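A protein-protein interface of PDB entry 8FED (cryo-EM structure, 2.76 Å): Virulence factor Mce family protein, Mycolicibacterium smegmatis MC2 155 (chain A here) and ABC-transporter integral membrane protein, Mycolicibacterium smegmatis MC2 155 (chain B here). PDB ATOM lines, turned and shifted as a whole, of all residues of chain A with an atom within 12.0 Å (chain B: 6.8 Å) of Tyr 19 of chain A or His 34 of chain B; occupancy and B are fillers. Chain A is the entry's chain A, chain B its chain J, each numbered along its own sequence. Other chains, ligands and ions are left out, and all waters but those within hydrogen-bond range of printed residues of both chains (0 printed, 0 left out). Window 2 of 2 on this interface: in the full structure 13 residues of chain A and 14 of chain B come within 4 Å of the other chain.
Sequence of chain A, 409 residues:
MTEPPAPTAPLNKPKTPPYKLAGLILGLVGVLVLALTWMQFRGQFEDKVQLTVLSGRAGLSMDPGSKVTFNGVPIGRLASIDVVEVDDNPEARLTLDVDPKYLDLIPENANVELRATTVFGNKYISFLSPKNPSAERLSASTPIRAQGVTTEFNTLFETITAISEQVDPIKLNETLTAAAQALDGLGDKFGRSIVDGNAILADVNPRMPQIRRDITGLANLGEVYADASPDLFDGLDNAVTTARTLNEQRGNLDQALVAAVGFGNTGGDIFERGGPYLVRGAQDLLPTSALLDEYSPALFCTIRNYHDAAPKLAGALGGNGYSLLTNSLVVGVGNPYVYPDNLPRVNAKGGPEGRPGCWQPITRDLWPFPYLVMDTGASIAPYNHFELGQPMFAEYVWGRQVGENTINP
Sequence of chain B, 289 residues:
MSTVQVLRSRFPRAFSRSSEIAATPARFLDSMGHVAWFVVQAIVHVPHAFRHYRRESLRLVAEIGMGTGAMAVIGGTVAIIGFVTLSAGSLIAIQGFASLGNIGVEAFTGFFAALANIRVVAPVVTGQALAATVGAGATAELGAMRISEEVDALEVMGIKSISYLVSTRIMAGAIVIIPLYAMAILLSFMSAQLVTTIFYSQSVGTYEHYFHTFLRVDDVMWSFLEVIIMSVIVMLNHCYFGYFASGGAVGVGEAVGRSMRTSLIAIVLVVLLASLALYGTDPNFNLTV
Of chain B, only Asp 30 (3.6 Å), Gly 33 (3.1 Å) and His 34 (3.98 Å) come within 4 Å of Tyr 19 of chain A.
Printed residues of chain B within 4 Å of Lys 20 of chain A: Leu 29.
Printed residues of chain B within 4 Å of Ala 22 of chain A: Gly 33 and Ala 36.
Asp 30 of chain B touches one residue of chain A.
No residue of chain A comes within 4 Å of Ser 31 of chain B.
Val 35 of chain B touches none of the printed residues of chain A.
No residue of chain A comes within 4 Å of Trp 37 of chain B.
No residue of chain A comes within 4 Å of Phe 244 of chain B.
The nearest residue of chain B that does not touch Tyr 19 of chain A is Trp 37 of chain B (4.2 Å).
The nearest residue of chain A that does not touch His 34 of chain B is Gly 23 of chain A (5.9 Å).
The nearest printed residue of chain B that does not touch Lys 20 of chain A is Gly 33 of chain B (5.1 Å).
Among the printed residues, pairs that only touch across the chains: Tyr 19 of chain A with Gly 33 of chain B, Lys 20 of chain A with Leu 29 of chain B, Gly 23 of chain A with Gly 33 of chain B, Ala 22 of chain A with Ala 36 of chain B, Tyr 19 of chain A with Asp 30 of chain B, Leu 26 of chain A with Ala 36 of chain B, Leu 26 of chain A with Met 32 of chain B, Ala 22 of chain A with Gly 33 of chain B and Tyr 19 of chain A with His 34 of chain B.
Among the printed residues, 9 pairs touch across the chains.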
ATOM      1  N   PRO A  18      14.915  -0.159  11.805  1.00  0.00           N
ATOM      2  CA  PRO A  18      16.056  -0.286  10.894  1.00  0.00           C
ATOM      3  C   PRO A  18      17.215   0.627  11.282  1.00  0.00           C
ATOM      4  O   PRO A  18      17.820   1.257  10.416  1.00  0.00           O
ATOM      5  CB  PRO A  18      15.466   0.126   9.545  1.00  0.00           C
ATOM      6  CG  PRO A  18      14.389   1.092   9.903  1.00  0.00           C
ATOM      7  CD  PRO A  18      13.801   0.587  11.194  1.00  0.00           C
ATOM      8  N   TYR A  19      17.510   0.695  12.582  1.00  0.00           N
ATOM      9  CA  TYR A  19      18.557   1.593  13.057  1.00  0.00           C
ATOM     10  C   TYR A  19      19.940   1.103  12.647  1.00  0.00           C
ATOM     11  O   TYR A  19      20.766   1.884  12.163  1.00  0.00           O
ATOM     12  CB  TYR A  19      18.463   1.754  14.575  1.00  0.00           C
ATOM     13  CG  TYR A  19      17.280   2.581  15.029  1.00  0.00           C
ATOM     14  CD1 TYR A  19      16.621   3.430  14.147  1.00  0.00           C
ATOM     15  CD2 TYR A  19      16.825   2.520  16.340  1.00  0.00           C
ATOM     16  CE1 TYR A  19      15.543   4.190  14.555  1.00  0.00           C
ATOM     17  CE2 TYR A  19      15.747   3.276  16.758  1.00  0.00           C
ATOM     18  CZ  TYR A  19      15.109   4.109  15.863  1.00  0.00           C
ATOM     19  OH  TYR A  19      14.035   4.865  16.273  1.00  0.00           O
ATOM     20  N   LYS A  20      20.217  -0.190  12.843  1.00  0.00           N
ATOM     21  CA  LYS A  20      21.545  -0.716  12.539  1.00  0.00           C
ATOM     22  C   LYS A  20      21.864  -0.595  11.052  1.00  0.00           C
ATOM     23  O   LYS A  20      22.982  -0.218  10.677  1.00  0.00           O
ATOM     24  CB  LYS A  20      21.645  -2.171  12.992  1.00  0.00           C
ATOM     25  CG  LYS A  20      21.145  -2.415  14.407  1.00  0.00           C
ATOM     26  CD  LYS A  20      21.369  -3.857  14.836  1.00  0.00           C
ATOM     27  CE  LYS A  20      22.847  -4.152  15.037  1.00  0.00           C
ATOM     28  NZ  LYS A  20      23.433  -3.330  16.132  1.00  0.00           N
ATOM     29  N   LEU A  21      20.891  -0.904  10.191  1.00  0.00           N
ATOM     30  CA  LEU A  21      21.098  -0.773   8.752  1.00  0.00           C
ATOM     31  C   LEU A  21      21.333   0.679   8.354  1.00  0.00           C
ATOM     32  O   LEU A  21      22.193   0.967   7.513  1.00  0.00           O
ATOM     33  CB  LEU A  21      19.900  -1.349   7.996  1.00  0.00           C
ATOM     34  CG  LEU A  21      19.966  -1.291   6.469  1.00  0.00           C
ATOM     35  CD1 LEU A  21      21.140  -2.107   5.951  1.00  0.00           C
ATOM     36  CD2 LEU A  21      18.661  -1.773   5.856  1.00  0.00           C
ATOM     37  N   ALA A  22      20.576   1.607   8.946  1.00  0.00           N
ATOM     38  CA  ALA A  22      20.771   3.024   8.653  1.00  0.00           C
ATOM     39  C   ALA A  22      22.150   3.500   9.094  1.00  0.00           C
ATOM     40  O   ALA A  22      22.800   4.279   8.387  1.00  0.00           O
ATOM     41  CB  ALA A  22      19.676   3.853   9.323  1.00  0.00           C
ATOM     42  N   GLY A  23      22.611   3.046  10.261  1.00  0.00           N
ATOM     43  CA  GLY A  23      23.952   3.399  10.701  1.00  0.00           C
ATOM     44  C   GLY A  23      25.032   2.839   9.795  1.00  0.00           C
ATOM     45  O   GLY A  23      26.022   3.514   9.501  1.00  0.00           O
ATOM     46  N   LEU A  24      24.858   1.591   9.345  1.00  0.00           N
ATOM     47  CA  LEU A  24      25.799   1.010   8.392  1.00  0.00           C
ATOM     48  C   LEU A  24      25.829   1.804   7.093  1.00  0.00           C
ATOM     49  O   LEU A  24      26.904   2.052   6.533  1.00  0.00           O
ATOM     50  CB  LEU A  24      25.445  -0.452   8.120  1.00  0.00           C
ATOM     51  CG  LEU A  24      25.662  -1.442   9.264  1.00  0.00           C
ATOM     52  CD1 LEU A  24      25.182  -2.829   8.871  1.00  0.00           C
ATOM     53  CD2 LEU A  24      27.127  -1.475   9.672  1.00  0.00           C
ATOM     54  N   ILE A  25      24.656   2.207   6.596  1.00  0.00           N
ATOM     55  CA  ILE A  25      24.593   2.996   5.368  1.00  0.00           C
ATOM     56  C   ILE A  25      25.282   4.343   5.558  1.00  0.00           C
ATOM     57  O   ILE A  25      26.021   4.803   4.682  1.00  0.00           O
ATOM     58  CB  ILE A  25      23.130   3.159   4.911  1.00  0.00           C
ATOM     59  CG1 ILE A  25      22.568   1.817   4.437  1.00  0.00           C
ATOM     60  CG2 ILE A  25      23.018   4.195   3.802  1.00  0.00           C
ATOM     61  CD1 ILE A  25      21.115   1.875   4.016  1.00  0.00           C
ATOM     62  N   LEU A  26      25.052   4.994   6.704  1.00  0.00           N
ATOM     63  CA  LEU A  26      25.693   6.281   6.968  1.00  0.00           C
ATOM     64  C   LEU A  26      27.210   6.144   7.027  1.00  0.00           C
ATOM     65  O   LEU A  26      27.940   6.967   6.457  1.00  0.00           O
ATOM     66  CB  LEU A  26      25.161   6.877   8.270  1.00  0.00           C
ATOM     67  CG  LEU A  26      25.801   8.194   8.719  1.00  0.00           C
ATOM     68  CD1 LEU A  26      25.509   9.306   7.724  1.00  0.00           C
ATOM     69  CD2 LEU A  26      25.332   8.580  10.114  1.00  0.00           C
ATOM     70  N   GLY A  27      27.703   5.113   7.719  1.00  0.00           N
ATOM     71  CA  GLY A  27      29.139   4.892   7.777  1.00  0.00           C
ATOM     72  C   GLY A  27      29.738   4.596   6.416  1.00  0.00           C
ATOM     73  O   GLY A  27      30.815   5.097   6.078  1.00  0.00           O
ATOM     74  N   LEU A  28      29.046   3.780   5.614  1.00  0.00           N
ATOM     75  CA  LEU A  28      29.518   3.479   4.267  1.00  0.00           C
ATOM     76  C   LEU A  28      29.557   4.735   3.407  1.00  0.00           C
ATOM     77  O   LEU A  28      30.502   4.937   2.636  1.00  0.00           O
ATOM     78  CB  LEU A  28      28.628   2.414   3.627  1.00  0.00           C
ATOM     79  CG  LEU A  28      29.071   1.865   2.269  1.00  0.00           C
ATOM     80  CD1 LEU A  28      30.394   1.129   2.397  1.00  0.00           C
ATOM     81  CD2 LEU A  28      28.002   0.958   1.682  1.00  0.00           C
ATOM     82  N   LEU B  29      26.816   2.341  17.571  1.00  0.00           N
ATOM     83  CA  LEU B  29      26.123   2.003  16.333  1.00  0.00           C
ATOM     84  C   LEU B  29      24.652   2.395  16.406  1.00  0.00           C
ATOM     85  O   LEU B  29      24.080   2.870  15.419  1.00  0.00           O
ATOM     86  CB  LEU B  29      26.272   0.510  16.038  1.00  0.00           C
ATOM     87  CG  LEU B  29      25.623   0.010  14.746  1.00  0.00           C
ATOM     88  CD1 LEU B  29      26.167   0.768  13.545  1.00  0.00           C
ATOM     89  CD2 LEU B  29      25.839  -1.486  14.583  1.00  0.00           C
ATOM     90  N   ASP B  30      24.025   2.196  17.568  1.00  0.00           N
ATOM     91  CA  ASP B  30      22.628   2.588  17.736  1.00  0.00           C
ATOM     92  C   ASP B  30      22.459   4.096  17.595  1.00  0.00           C
ATOM     93  O   ASP B  30      21.505   4.564  16.962  1.00  0.00           O
ATOM     94  CB  ASP B  30      22.111   2.108  19.093  1.00  0.00           C
ATOM     95  CG  ASP B  30      20.601   2.211  19.216  1.00  0.00           C
ATOM     96  OD1 ASP B  30      19.931   2.482  18.198  1.00  0.00           O
ATOM     97  OD2 ASP B  30      20.082   2.019  20.336  1.00  0.00           O
ATOM     98  N   SER B  31      23.370   4.875  18.185  1.00  0.00           N
ATOM     99  CA  SER B  31      23.293   6.328  18.064  1.00  0.00           C
ATOM    100  C   SER B  31      23.518   6.779  16.626  1.00  0.00           C
ATOM    101  O   SER B  31      22.835   7.693  16.142  1.00  0.00           O
ATOM    102  CB  SER B  31      24.308   6.987  18.999  1.00  0.00           C
ATOM    103  OG  SER B  31      24.235   8.399  18.914  1.00  0.00           O
ATOM    104  N   MET B  32      24.478   6.159  15.931  1.00  0.00           N
ATOM    105  CA  MET B  32      24.693   6.482  14.524  1.00  0.00           C
ATOM    106  C   MET B  32      23.460   6.156  13.692  1.00  0.00           C
ATOM    107  O   MET B  32      23.078   6.926  12.805  1.00  0.00           O
ATOM    108  CB  MET B  32      25.912   5.737  13.984  1.00  0.00           C
ATOM    109  CG  MET B  32      27.241   6.239  14.515  1.00  0.00           C
ATOM    110  SD  MET B  32      28.627   5.613  13.550  1.00  0.00           S
ATOM    111  CE  MET B  32      28.283   6.344  11.951  1.00  0.00           C
ATOM    112  N   GLY B  33      22.824   5.018  13.965  1.00  0.00           N
ATOM    113  CA  GLY B  33      21.608   4.679  13.249  1.00  0.00           C
ATOM    114  C   GLY B  33      20.474   5.643  13.535  1.00  0.00           C
ATOM    115  O   GLY B  33      19.709   6.000  12.637  1.00  0.00           O
ATOM    116  N   HIS B  34      20.350   6.074  14.792  1.00  0.00           N
ATOM    117  CA  HIS B  34      19.307   7.028  15.153  1.00  0.00           C
ATOM    118  C   HIS B  34      19.506   8.364  14.445  1.00  0.00           C
ATOM    119  O   HIS B  34      18.554   8.937  13.900  1.00  0.00           O
ATOM    120  CB  HIS B  34      19.279   7.218  16.670  1.00  0.00           C
ATOM    121  CG  HIS B  34      18.112   8.018  17.158  1.00  0.00           C
ATOM    122  ND1 HIS B  34      16.806   7.636  16.942  1.00  0.00           N
ATOM    123  CD2 HIS B  34      18.055   9.176  17.857  1.00  0.00           C
ATOM    124  CE1 HIS B  34      15.994   8.526  17.483  1.00  0.00           C
ATOM    125  NE2 HIS B  34      16.726   9.470  18.046  1.00  0.00           N
ATOM    126  N   VAL B  35      20.741   8.874  14.430  1.00  0.00           N
ATOM    127  CA  VAL B  35      20.981  10.154  13.766  1.00  0.00           C
ATOM    128  C   VAL B  35      20.829  10.016  12.251  1.00  0.00           C
ATOM    129  O   VAL B  35      20.337  10.933  11.581  1.00  0.00           O
ATOM    130  CB  VAL B  35      22.349  10.745  14.173  1.00  0.00           C
ATOM    131  CG1 VAL B  35      23.504   9.874  13.734  1.00  0.00           C
ATOM    132  CG2 VAL B  35      22.507  12.160  13.624  1.00  0.00           C
ATOM    133  N   ALA B  36      21.232   8.870  11.687  1.00  0.00           N
ATOM    134  CA  ALA B  36      21.030   8.643  10.259  1.00  0.00           C
ATOM    135  C   ALA B  36      19.548   8.601   9.907  1.00  0.00           C
ATOM    136  O   ALA B  36      19.125   9.183   8.902  1.00  0.00           O
ATOM    137  CB  ALA B  36      21.721   7.348   9.831  1.00  0.00           C
ATOM    138  N   TRP B  37      18.744   7.918  10.725  1.00  0.00           N
ATOM    139  CA  TRP B  37      17.305   7.895  10.490  1.00  0.00           C
ATOM    140  C   TRP B  37      16.714   9.292  10.605  1.00  0.00           C
ATOM    141  O   TRP B  37      15.850   9.674   9.806  1.00  0.00           O
ATOM    142  CB  TRP B  37      16.623   6.940  11.469  1.00  0.00           C
ATOM    143  CG  TRP B  37      15.125   6.990  11.400  1.00  0.00           C
ATOM    144  CD1 TRP B  37      14.318   6.264  10.572  1.00  0.00           C
ATOM    145  CD2 TRP B  37      14.253   7.809  12.190  1.00  0.00           C
ATOM    146  NE1 TRP B  37      13.002   6.582  10.796  1.00  0.00           N
ATOM    147  CE2 TRP B  37      12.935   7.529  11.784  1.00  0.00           C
ATOM    148  CE3 TRP B  37      14.462   8.755  13.198  1.00  0.00           C
ATOM    149  CZ2 TRP B  37      11.830   8.158  12.352  1.00  0.00           C
ATOM    150  CZ3 TRP B  37      13.364   9.378  13.761  1.00  0.00           C
ATOM    151  CH2 TRP B  37      12.065   9.077  13.338  1.00  0.00           C
ATOM    152  N   PHE B  38      17.168  10.068  11.594  1.00  0.00           N
ATOM    153  CA  PHE B  38      16.665  11.427  11.761  1.00  0.00           C
ATOM    154  C   PHE B  38      16.969  12.282  10.537  1.00  0.00           C
ATOM    155  O   PHE B  38      16.091  12.987  10.030  1.00  0.00           O
ATOM    156  CB  PHE B  38      17.259  12.059  13.021  1.00  0.00           C
ATOM    157  CG  PHE B  38      16.899  13.509  13.201  1.00  0.00           C
ATOM    158  CD1 PHE B  38      15.707  13.866  13.804  1.00  0.00           C
ATOM    159  CD2 PHE B  38      17.752  14.512  12.773  1.00  0.00           C
ATOM    160  CE1 PHE B  38      15.370  15.193  13.972  1.00  0.00           C
ATOM    161  CE2 PHE B  38      17.416  15.840  12.932  1.00  0.00           C
ATOM    162  CZ  PHE B  38      16.227  16.180  13.538  1.00  0.00           C
ATOM    163  N   VAL B  39      18.211  12.232  10.044  1.00  0.00           N
ATOM    164  CA  VAL B  39      18.573  13.088   8.915  1.00  0.00           C
ATOM    165  C   VAL B  39      17.863  12.628   7.644  1.00  0.00           C
ATOM    166  O   VAL B  39      17.430  13.455   6.831  1.00  0.00           O
ATOM    167  CB  VAL B  39      20.103  13.174   8.737  1.00  0.00           C
ATOM    168  CG1 VAL B  39      20.748  13.785   9.973  1.00  0.00           C
ATOM    169  CG2 VAL B  39      20.721  11.828   8.424  1.00  0.00           C
ATOM    170  N   TYR B 240      18.884  17.873  15.347  1.00  0.00           N
ATOM    171  CA  TYR B 240      18.946  16.569  16.000  1.00  0.00           C
ATOM    172  C   TYR B 240      19.162  16.712  17.498  1.00  0.00           C
ATOM    173  O   TYR B 240      18.520  16.018  18.294  1.00  0.00           O
ATOM    174  CB  TYR B 240      20.053  15.713  15.391  1.00  0.00           C
ATOM    175  CG  TYR B 240      20.285  14.420  16.142  1.00  0.00           C
ATOM    176  CD1 TYR B 240      19.433  13.338  15.981  1.00  0.00           C
ATOM    177  CD2 TYR B 240      21.360  14.282  17.011  1.00  0.00           C
ATOM    178  CE1 TYR B 240      19.640  12.157  16.666  1.00  0.00           C
ATOM    179  CE2 TYR B 240      21.574  13.106  17.699  1.00  0.00           C
ATOM    180  CZ  TYR B 240      20.711  12.047  17.522  1.00  0.00           C
ATOM    181  OH  TYR B 240      20.921  10.872  18.204  1.00  0.00           O
ATOM    182  N   TYR B 243      15.890  18.395  19.071  1.00  0.00           N
ATOM    183  CA  TYR B 243      14.615  17.707  18.905  1.00  0.00           C
ATOM    184  C   TYR B 243      14.432  16.619  19.953  1.00  0.00           C
ATOM    185  O   TYR B 243      13.319  16.408  20.448  1.00  0.00           O
ATOM    186  CB  TYR B 243      14.526  17.127  17.493  1.00  0.00           C
ATOM    187  CG  TYR B 243      13.212  16.456  17.161  1.00  0.00           C
ATOM    188  CD1 TYR B 243      12.108  17.201  16.773  1.00  0.00           C
ATOM    189  CD2 TYR B 243      13.084  15.076  17.215  1.00  0.00           C
ATOM    190  CE1 TYR B 243      10.909  16.591  16.463  1.00  0.00           C
ATOM    191  CE2 TYR B 243      11.891  14.457  16.907  1.00  0.00           C
ATOM    192  CZ  TYR B 243      10.807  15.218  16.531  1.00  0.00           C
ATOM    193  OH  TYR B 243       9.617  14.600  16.224  1.00  0.00           O
ATOM    194  N   PHE B 244      15.509  15.921  20.308  1.00  0.00           N
ATOM    195  CA  PHE B 244      15.462  14.839  21.287  1.00  0.00           C
ATOM    196  C   PHE B 244      16.013  15.272  22.638  1.00  0.00           C
ATOM    197  O   PHE B 244      16.657  14.485  23.336  1.00  0.00           O
ATOM    198  CB  PHE B 244      16.218  13.621  20.768  1.00  0.00           C
ATOM    199  CG  PHE B 244      15.642  13.040  19.510  1.00  0.00           C
ATOM    200  CD1 PHE B 244      14.495  12.268  19.551  1.00  0.00           C
ATOM    201  CD2 PHE B 244      16.253  13.257  18.288  1.00  0.00           C
ATOM    202  CE1 PHE B 244      13.964  11.730  18.396  1.00  0.00           C
ATOM    203  CE2 PHE B 244      15.727  12.720  17.130  1.00  0.00           C
ATOM    204  CZ  PHE B 244      14.581  11.955  17.186  1.00  0.00           C
